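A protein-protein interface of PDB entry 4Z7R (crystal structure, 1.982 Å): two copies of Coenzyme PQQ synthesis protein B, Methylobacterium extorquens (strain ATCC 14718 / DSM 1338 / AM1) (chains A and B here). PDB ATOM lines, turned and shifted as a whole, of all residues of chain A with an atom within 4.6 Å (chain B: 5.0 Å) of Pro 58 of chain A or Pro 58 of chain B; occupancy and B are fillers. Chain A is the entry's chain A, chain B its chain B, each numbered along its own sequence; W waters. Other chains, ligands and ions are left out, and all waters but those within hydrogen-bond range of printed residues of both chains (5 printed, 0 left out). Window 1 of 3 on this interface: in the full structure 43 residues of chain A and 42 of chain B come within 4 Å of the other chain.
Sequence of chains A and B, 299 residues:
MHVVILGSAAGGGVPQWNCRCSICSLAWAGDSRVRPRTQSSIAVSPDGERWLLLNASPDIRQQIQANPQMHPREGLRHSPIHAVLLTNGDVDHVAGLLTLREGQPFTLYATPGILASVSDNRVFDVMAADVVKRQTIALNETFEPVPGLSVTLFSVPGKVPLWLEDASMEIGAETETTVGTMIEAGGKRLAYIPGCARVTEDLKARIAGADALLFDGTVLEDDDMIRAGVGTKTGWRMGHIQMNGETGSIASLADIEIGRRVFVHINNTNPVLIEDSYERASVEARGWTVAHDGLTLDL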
ATOM      1  N   GLN A  39      10.299   2.830  30.556  1.00  0.00           N
ATOM      2  CA  GLN A  39       9.595   1.953  29.622  1.00  0.00           C
ATOM      3  C   GLN A  39      10.478   0.926  28.915  1.00  0.00           C
ATOM      4  O   GLN A  39      11.663   1.159  28.684  1.00  0.00           O
ATOM      5  CB  GLN A  39       8.838   2.793  28.592  1.00  0.00           C
ATOM      6  CG  GLN A  39       7.626   3.501  29.201  1.00  0.00           C
ATOM      7  CD  GLN A  39       7.139   4.670  28.374  1.00  0.00           C
ATOM      8  OE1 GLN A  39       6.220   4.535  27.568  1.00  0.00           O
ATOM      9  NE2 GLN A  39       7.747   5.833  28.578  1.00  0.00           N
ATOM     10  N   ALA A  56      13.811   0.988  21.777  1.00  0.00           N
ATOM     11  CA  ALA A  56      14.274   2.332  22.109  1.00  0.00           C
ATOM     12  C   ALA A  56      13.115   3.143  22.684  1.00  0.00           C
ATOM     13  O   ALA A  56      12.286   3.673  21.945  1.00  0.00           O
ATOM     14  CB  ALA A  56      14.876   3.039  20.908  1.00  0.00           C
ATOM     15  N   SER A  57      13.059   3.217  24.010  1.00  0.00           N
ATOM     16  CA  SER A  57      11.904   3.765  24.717  1.00  0.00           C
ATOM     17  C   SER A  57      11.945   5.292  24.822  1.00  0.00           C
ATOM     18  O   SER A  57      13.000   5.897  24.647  1.00  0.00           O
ATOM     19  CB  SER A  57      11.817   3.139  26.113  1.00  0.00           C
ATOM     20  OG  SER A  57      12.389   3.990  27.088  1.00  0.00           O
ATOM     21  N   PRO A  58      10.789   5.923  25.107  1.00  0.00           N
ATOM     22  CA  PRO A  58      10.760   7.377  25.301  1.00  0.00           C
ATOM     23  C   PRO A  58      11.677   7.852  26.433  1.00  0.00           C
ATOM     24  O   PRO A  58      12.012   9.035  26.489  1.00  0.00           O
ATOM     25  CB  PRO A  58       9.291   7.657  25.640  1.00  0.00           C
ATOM     26  CG  PRO A  58       8.542   6.529  25.012  1.00  0.00           C
ATOM     27  CD  PRO A  58       9.437   5.339  25.172  1.00  0.00           C
ATOM     28  N   ASP A  59      12.062   6.939  27.321  1.00  0.00           N
ATOM     29  CA  ASP A  59      12.906   7.269  28.466  1.00  0.00           C
ATOM     30  C   ASP A  59      14.391   7.024  28.202  1.00  0.00           C
ATOM     31  O   ASP A  59      15.193   7.046  29.131  1.00  0.00           O
ATOM     32  CB  ASP A  59      12.491   6.445  29.685  1.00  0.00           C
ATOM     33  CG  ASP A  59      11.036   6.643  30.063  1.00  0.00           C
ATOM     34  OD1 ASP A  59      10.681   7.752  30.510  1.00  0.00           O
ATOM     35  OD2 ASP A  59      10.251   5.682  29.918  1.00  0.00           O
ATOM     36  N   ILE A  60      14.752   6.790  26.945  1.00  0.00           N
ATOM     37  CA  ILE A  60      16.075   6.254  26.625  1.00  0.00           C
ATOM     38  C   ILE A  60      17.220   7.134  27.130  1.00  0.00           C
ATOM     39  O   ILE A  60      18.271   6.627  27.523  1.00  0.00           O
ATOM     40  CB  ILE A  60      16.231   6.025  25.103  1.00  0.00           C
ATOM     41  CG1 ILE A  60      17.558   5.325  24.794  1.00  0.00           C
ATOM     42  CG2 ILE A  60      16.116   7.336  24.338  1.00  0.00           C
ATOM     43  CD1 ILE A  60      17.735   4.966  23.338  1.00  0.00           C
ATOM     44  N   VAL A  91       4.869   2.721  20.325  1.00  0.00           N
ATOM     45  CA  VAL A  91       5.541   3.983  20.621  1.00  0.00           C
ATOM     46  C   VAL A  91       6.553   3.833  21.755  1.00  0.00           C
ATOM     47  O   VAL A  91       7.625   4.441  21.721  1.00  0.00           O
ATOM     48  CB  VAL A  91       4.514   5.093  20.952  1.00  0.00           C
ATOM     49  CG1 VAL A  91       5.064   6.086  21.961  1.00  0.00           C
ATOM     50  CG2 VAL A  91       4.115   5.806  19.682  1.00  0.00           C
ATOM     51  N   ASP A  92       6.255   2.981  22.731  1.00  0.00           N
ATOM     52  CA  ASP A  92       7.181   2.821  23.849  1.00  0.00           C
ATOM     53  C   ASP A  92       8.420   2.013  23.448  1.00  0.00           C
ATOM     54  O   ASP A  92       9.361   1.890  24.228  1.00  0.00           O
ATOM     55  CB  ASP A  92       6.488   2.164  25.050  1.00  0.00           C
ATOM     56  CG  ASP A  92       5.949   0.782  24.739  1.00  0.00           C
ATOM     57  OD1 ASP A  92       5.701   0.492  23.556  1.00  0.00           O
ATOM     58  OD2 ASP A  92       5.780  -0.018  25.681  1.00  0.00           O
ATOM     59  N   ALA A  95       9.997   5.318  20.129  1.00  0.00           N
ATOM     60  CA  ALA A  95      10.126   6.762  20.351  1.00  0.00           C
ATOM     61  C   ALA A  95      11.559   7.175  20.685  1.00  0.00           C
ATOM     62  O   ALA A  95      11.992   8.274  20.335  1.00  0.00           O
ATOM     63  CB  ALA A  95       9.181   7.220  21.454  1.00  0.00           C
ATOM     64  N   GLY A  96      12.296   6.287  21.343  1.00  0.00           N
ATOM     65  CA  GLY A  96      13.673   6.563  21.714  1.00  0.00           C
ATOM     66  C   GLY A  96      14.624   6.795  20.555  1.00  0.00           C
ATOM     67  O   GLY A  96      15.695   7.383  20.728  1.00  0.00           O
ATOM     68  N   THR A  99      15.962  10.211  19.862  1.00  0.00           N
ATOM     69  CA  THR A  99      17.045  10.686  20.718  1.00  0.00           C
ATOM     70  C   THR A  99      18.412  10.307  20.138  1.00  0.00           C
ATOM     71  O   THR A  99      19.401  11.017  20.324  1.00  0.00           O
ATOM     72  CB  THR A  99      16.887  10.120  22.153  1.00  0.00           C
ATOM     73  OG1 THR A  99      15.895  10.875  22.854  1.00  0.00           O
ATOM     74  CG2 THR A  99      18.194  10.171  22.935  1.00  0.00           C
ATOM     75  N   ARG A 101      20.160  10.655  17.526  1.00  0.00           N
ATOM     76  CA  ARG A 101      20.183  11.392  16.264  1.00  0.00           C
ATOM     77  C   ARG A 101      21.468  12.166  15.946  1.00  0.00           C
ATOM     78  O   ARG A 101      21.703  12.517  14.790  1.00  0.00           O
ATOM     79  CB  ARG A 101      19.008  12.369  16.232  1.00  0.00           C
ATOM     80  CG  ARG A 101      19.052  13.424  17.323  1.00  0.00           C
ATOM     81  CD  ARG A 101      17.864  14.372  17.231  1.00  0.00           C
ATOM     82  NE  ARG A 101      17.942  15.442  18.223  1.00  0.00           N
ATOM     83  CZ  ARG A 101      17.447  15.363  19.454  1.00  0.00           C
ATOM     84  NH1 ARG A 101      17.576  16.385  20.287  1.00  0.00           N
ATOM     85  NH2 ARG A 101      16.819  14.264  19.852  1.00  0.00           N
ATOM     86  N   GLN B  39      15.991  18.708  27.897  1.00  0.00           N
ATOM     87  CA  GLN B  39      15.964  19.620  26.760  1.00  0.00           C
ATOM     88  C   GLN B  39      14.851  20.665  26.890  1.00  0.00           C
ATOM     89  O   GLN B  39      13.782  20.390  27.435  1.00  0.00           O
ATOM     90  CB  GLN B  39      15.831  18.816  25.466  1.00  0.00           C
ATOM     91  CG  GLN B  39      17.119  18.052  25.135  1.00  0.00           C
ATOM     92  CD  GLN B  39      16.911  16.893  24.179  1.00  0.00           C
ATOM     93  OE1 GLN B  39      17.098  17.027  22.969  1.00  0.00           O
ATOM     94  NE2 GLN B  39      16.539  15.739  24.723  1.00  0.00           N
ATOM     95  N   ALA B  56       7.279  20.230  23.591  1.00  0.00           N
ATOM     96  CA  ALA B  56       7.219  18.936  24.253  1.00  0.00           C
ATOM     97  C   ALA B  56       8.508  18.180  23.961  1.00  0.00           C
ATOM     98  O   ALA B  56       8.656  17.553  22.910  1.00  0.00           O
ATOM     99  CB  ALA B  56       6.006  18.145  23.789  1.00  0.00           C
ATOM    100  N   SER B  57       9.471  18.291  24.870  1.00  0.00           N
ATOM    101  CA  SER B  57      10.810  17.751  24.642  1.00  0.00           C
ATOM    102  C   SER B  57      10.869  16.237  24.806  1.00  0.00           C
ATOM    103  O   SER B  57       9.982  15.637  25.414  1.00  0.00           O
ATOM    104  CB  SER B  57      11.821  18.418  25.577  1.00  0.00           C
ATOM    105  OG  SER B  57      11.910  17.725  26.810  1.00  0.00           O
ATOM    106  N   PRO B  58      11.917  15.622  24.264  1.00  0.00           N
ATOM    107  CA  PRO B  58      12.082  14.169  24.394  1.00  0.00           C
ATOM    108  C   PRO B  58      12.136  13.697  25.845  1.00  0.00           C
ATOM    109  O   PRO B  58      11.917  12.517  26.117  1.00  0.00           O
ATOM    110  CB  PRO B  58      13.420  13.905  23.692  1.00  0.00           C
ATOM    111  CG  PRO B  58      13.556  15.024  22.725  1.00  0.00           C
ATOM    112  CD  PRO B  58      12.971  16.214  23.420  1.00  0.00           C
ATOM    113  N   ASP B  59      12.429  14.614  26.761  1.00  0.00           N
ATOM    114  CA  ASP B  59      12.557  14.279  28.174  1.00  0.00           C
ATOM    115  C   ASP B  59      11.281  14.518  28.977  1.00  0.00           C
ATOM    116  O   ASP B  59      11.319  14.510  30.204  1.00  0.00           O
ATOM    117  CB  ASP B  59      13.688  15.088  28.808  1.00  0.00           C
ATOM    118  CG  ASP B  59      15.022  14.870  28.130  1.00  0.00           C
ATOM    119  OD1 ASP B  59      15.565  13.751  28.229  1.00  0.00           O
ATOM    120  OD2 ASP B  59      15.540  15.829  27.514  1.00  0.00           O
ATOM    121  N   ILE B  60      10.163  14.742  28.293  1.00  0.00           N
ATOM    122  CA  ILE B  60       8.968  15.266  28.956  1.00  0.00           C
ATOM    123  C   ILE B  60       8.475  14.375  30.104  1.00  0.00           C
ATOM    124  O   ILE B  60       7.951  14.883  31.095  1.00  0.00           O
ATOM    125  CB  ILE B  60       7.815  15.490  27.947  1.00  0.00           C
ATOM    126  CG1 ILE B  60       6.645  16.219  28.613  1.00  0.00           C
ATOM    127  CG2 ILE B  60       7.367  14.178  27.322  1.00  0.00           C
ATOM    128  CD1 ILE B  60       5.536  16.564  27.660  1.00  0.00           C
ATOM    129  N   VAL B  91      12.584  18.104  16.078  1.00  0.00           N
ATOM    130  CA  VAL B  91      12.346  16.865  16.810  1.00  0.00           C
ATOM    131  C   VAL B  91      12.402  17.060  18.328  1.00  0.00           C
ATOM    132  O   VAL B  91      11.647  16.428  19.067  1.00  0.00           O
ATOM    133  CB  VAL B  91      13.360  15.771  16.379  1.00  0.00           C
ATOM    134  CG1 VAL B  91      14.793  16.269  16.524  1.00  0.00           C
ATOM    135  CG2 VAL B  91      13.149  14.485  17.160  1.00  0.00           C
ATOM    136  N   ASP B  92      13.273  17.948  18.797  1.00  0.00           N
ATOM    137  CA  ASP B  92      13.389  18.200  20.231  1.00  0.00           C
ATOM    138  C   ASP B  92      12.245  19.073  20.763  1.00  0.00           C
ATOM    139  O   ASP B  92      12.131  19.294  21.970  1.00  0.00           O
ATOM    140  CB  ASP B  92      14.746  18.830  20.560  1.00  0.00           C
ATOM    141  CG  ASP B  92      14.965  20.152  19.861  1.00  0.00           C
ATOM    142  OD1 ASP B  92      14.313  20.403  18.828  1.00  0.00           O
ATOM    143  OD2 ASP B  92      15.805  20.937  20.345  1.00  0.00           O
ATOM    144  N   ALA B  95       9.008  15.630  20.015  1.00  0.00           N
ATOM    145  CA  ALA B  95       9.161  14.220  20.383  1.00  0.00           C
ATOM    146  C   ALA B  95       8.386  13.868  21.649  1.00  0.00           C
ATOM    147  O   ALA B  95       7.917  12.739  21.805  1.00  0.00           O
ATOM    148  CB  ALA B  95      10.631  13.870  20.559  1.00  0.00           C
ATOM    149  N   GLY B  96       8.258  14.837  22.548  1.00  0.00           N
ATOM    150  CA  GLY B  96       7.519  14.645  23.783  1.00  0.00           C
ATOM    151  C   GLY B  96       6.040  14.362  23.597  1.00  0.00           C
ATOM    152  O   GLY B  96       5.386  13.834  24.497  1.00  0.00           O
ATOM    153  N   THR B  99       4.675  10.949  24.259  1.00  0.00           N
ATOM    154  CA  THR B  99       4.487  10.549  25.653  1.00  0.00           C
ATOM    155  C   THR B  99       3.081  10.939  26.143  1.00  0.00           C
ATOM    156  O   THR B  99       2.489  10.263  26.986  1.00  0.00           O
ATOM    157  CB  THR B  99       5.582  11.177  26.554  1.00  0.00           C
ATOM    158  OG1 THR B  99       6.801  10.433  26.415  1.00  0.00           O
ATOM    159  CG2 THR B  99       5.177  11.194  28.021  1.00  0.00           C
ATOM    160  N   ARG B 101       0.020  10.526  25.371  1.00  0.00           N
ATOM    161  CA  ARG B 101      -0.847   9.764  24.473  1.00  0.00           C
ATOM    162  C   ARG B 101      -2.005   9.006  25.124  1.00  0.00           C
ATOM    163  O   ARG B 101      -2.962   8.638  24.444  1.00  0.00           O
ATOM    164  CB  ARG B 101       0.005   8.763  23.685  1.00  0.00           C
ATOM    165  CG  ARG B 101       0.709   7.725  24.551  1.00  0.00           C
ATOM    166  CD  ARG B 101       1.549   6.767  23.709  1.00  0.00           C
ATOM    167  NE  ARG B 101       2.160   5.722  24.524  1.00  0.00           N
ATOM    168  CZ  ARG B 101       3.342   5.834  25.123  1.00  0.00           C
ATOM    169  NH1 ARG B 101       3.811   4.832  25.851  1.00  0.00           N
ATOM    170  NH2 ARG B 101       4.053   6.950  25.001  1.00  0.00           N
HETATM  171  O   HOH W   1      11.064  10.538  24.055  1.00  0.00           O
HETATM  172  O   HOH W   2      10.400  11.453  28.231  1.00  0.00           O
HETATM  173  O   HOH W   3      16.892  13.593  22.669  1.00  0.00           O
HETATM  174  O   HOH W   4      14.439  10.291  27.067  1.00  0.00           O
HETATM  175  O   HOH W   5       5.996   7.832  27.267  1.00  0.00           O
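The guanidinium group (NH1) of Arg 101 of chain A is in hydrogen-bond range of the side-chain amide oxygen (OE1) of Gln 39 of chain B, at 2.8 Å.
The guanidinium group of Arg 101 of chain B sits at hydrogen-bond distance from the side-chain amide oxygen of Gln 39 of chain A.
The backbone carbonyl oxygen (O) of Gln 39 of chain A sits close to the side-chain hydroxyl (OG) of Ser 57 of chain A, at 3.3 Å.
The side-chain hydroxyl of Ser 57 of chain B sits at hydrogen-bond distance from the backbone carbonyl oxygen of Gln 39 of chain B.
NE2 of Gln 39 of chain A is in hydrogen-bond range of OD2 of Asp 59 of chain A, 2.8 Å away.
OD2 of Asp 59 of chain B is in hydrogen-bond range of N of Gln 39 of chain B, at 2.9 Å.
Among the printed residues, pairs that only touch across the chains: Pro 58 of chain A with Pro 58 of chain B (3.5 Å), Pro 58 of chain A with Thr 99 of chain B (3.8 Å), Val 91 of chain A with Arg 101 of chain B (3.3 Å), Asp 92 of chain A with Arg 101 of chain B (3.9 Å), Arg 101 of chain A with Val 91 of chain B (3.7 Å) and Arg 101 of chain A with Asp 92 of chain B (3.7 Å).
Of the printed residues of chain B, Gln 39 of chain A touches Arg 101.
Pro 58 of chain A touches just these residues of chain B: Pro 58 (3.5 Å) and Thr 99 (3.8 Å).
Asp 59 of chain A touches none of the printed residues of chain B.
Of the printed residues of chain B, Val 91 of chain A touches Arg 101.
Ser 57 of chain B touches none of the printed residues of chain A.
Of the printed residues of chain A, Pro 58 of chain B touches Pro 58 (3.5 Å).
Printed residues of chain A within 4 Å of Val 91 of chain B: Arg 101.
Hydrophobic or aromatic side chains of chain B that line the printed part of chain A: Val 91.
Of the 12 printed residues of chain A, 5 touch a printed residue of chain B.
Printed residues of chain A that touch a printed residue of chain B: Gln 39, Pro 58, Val 91, Asp 92 and Arg 101.
Hydrophobic or aromatic side chains of chain A within 4 Å of the printed part of chain B: Pro 58 and Val 91.
Pro 58 of chain B touches its own counterpart, Pro 58 of chain A.
Pro 58 of chain A touches Thr 99 of chain B, but with the chains exchanged Thr 99 of chain A does not touch Pro 58 of chain B (4.001 Å).
Val 91 of chain A touches Arg 101 of chain B, and with the chains exchanged Arg 101 of chain A touches Val 91 of chain B.
Asp 92 of chain A touches Arg 101 of chain B, and with the chains exchanged Arg 101 of chain A touches Asp 92 of chain B.
Positions printed for both chains: 39, 56, 57, 58, 59, 60, 91, 92, 95, 96, 99 and 101.
Water W4 bridges the backbone carbonyl oxygen of Pro 58 of chain A and the backbone carbonyl oxygen of Pro 58 of chain B.
Water W2 lies within hydrogen-bond range of the backbone carbonyl oxygen (O) of Pro 58 of chain B (2.8 Å), the backbone NH (N) of Ile 60 of chain B (3.3 Å) and the backbone carbonyl oxygen (O) of Pro 58 of chain A (3.4 Å).
Water W5 lies within hydrogen-bond range of the side-chain hydroxyl (OG1) of Thr 99 of chain B, the side-chain amide nitrogen (NE2) of Gln 39 of chain A and the guanidinium group (NH2) of Arg 101 of chain B.
Water W3 lies within hydrogen-bond range of the guanidinium group (NH2) of Arg 101 of chain A (2.9 Å), the side-chain hydroxyl (OG1) of Thr 99 of chain A (2.9 Å) and the side-chain amide nitrogen (NE2) of Gln 39 of chain B (3.0 Å).
Water W1 lies within hydrogen-bond range of the backbone carbonyl oxygen (O) of Pro 58 of chain B (3.0 Å) and the backbone carbonyl oxygen (O) of Pro 58 of chain A (3.0 Å).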
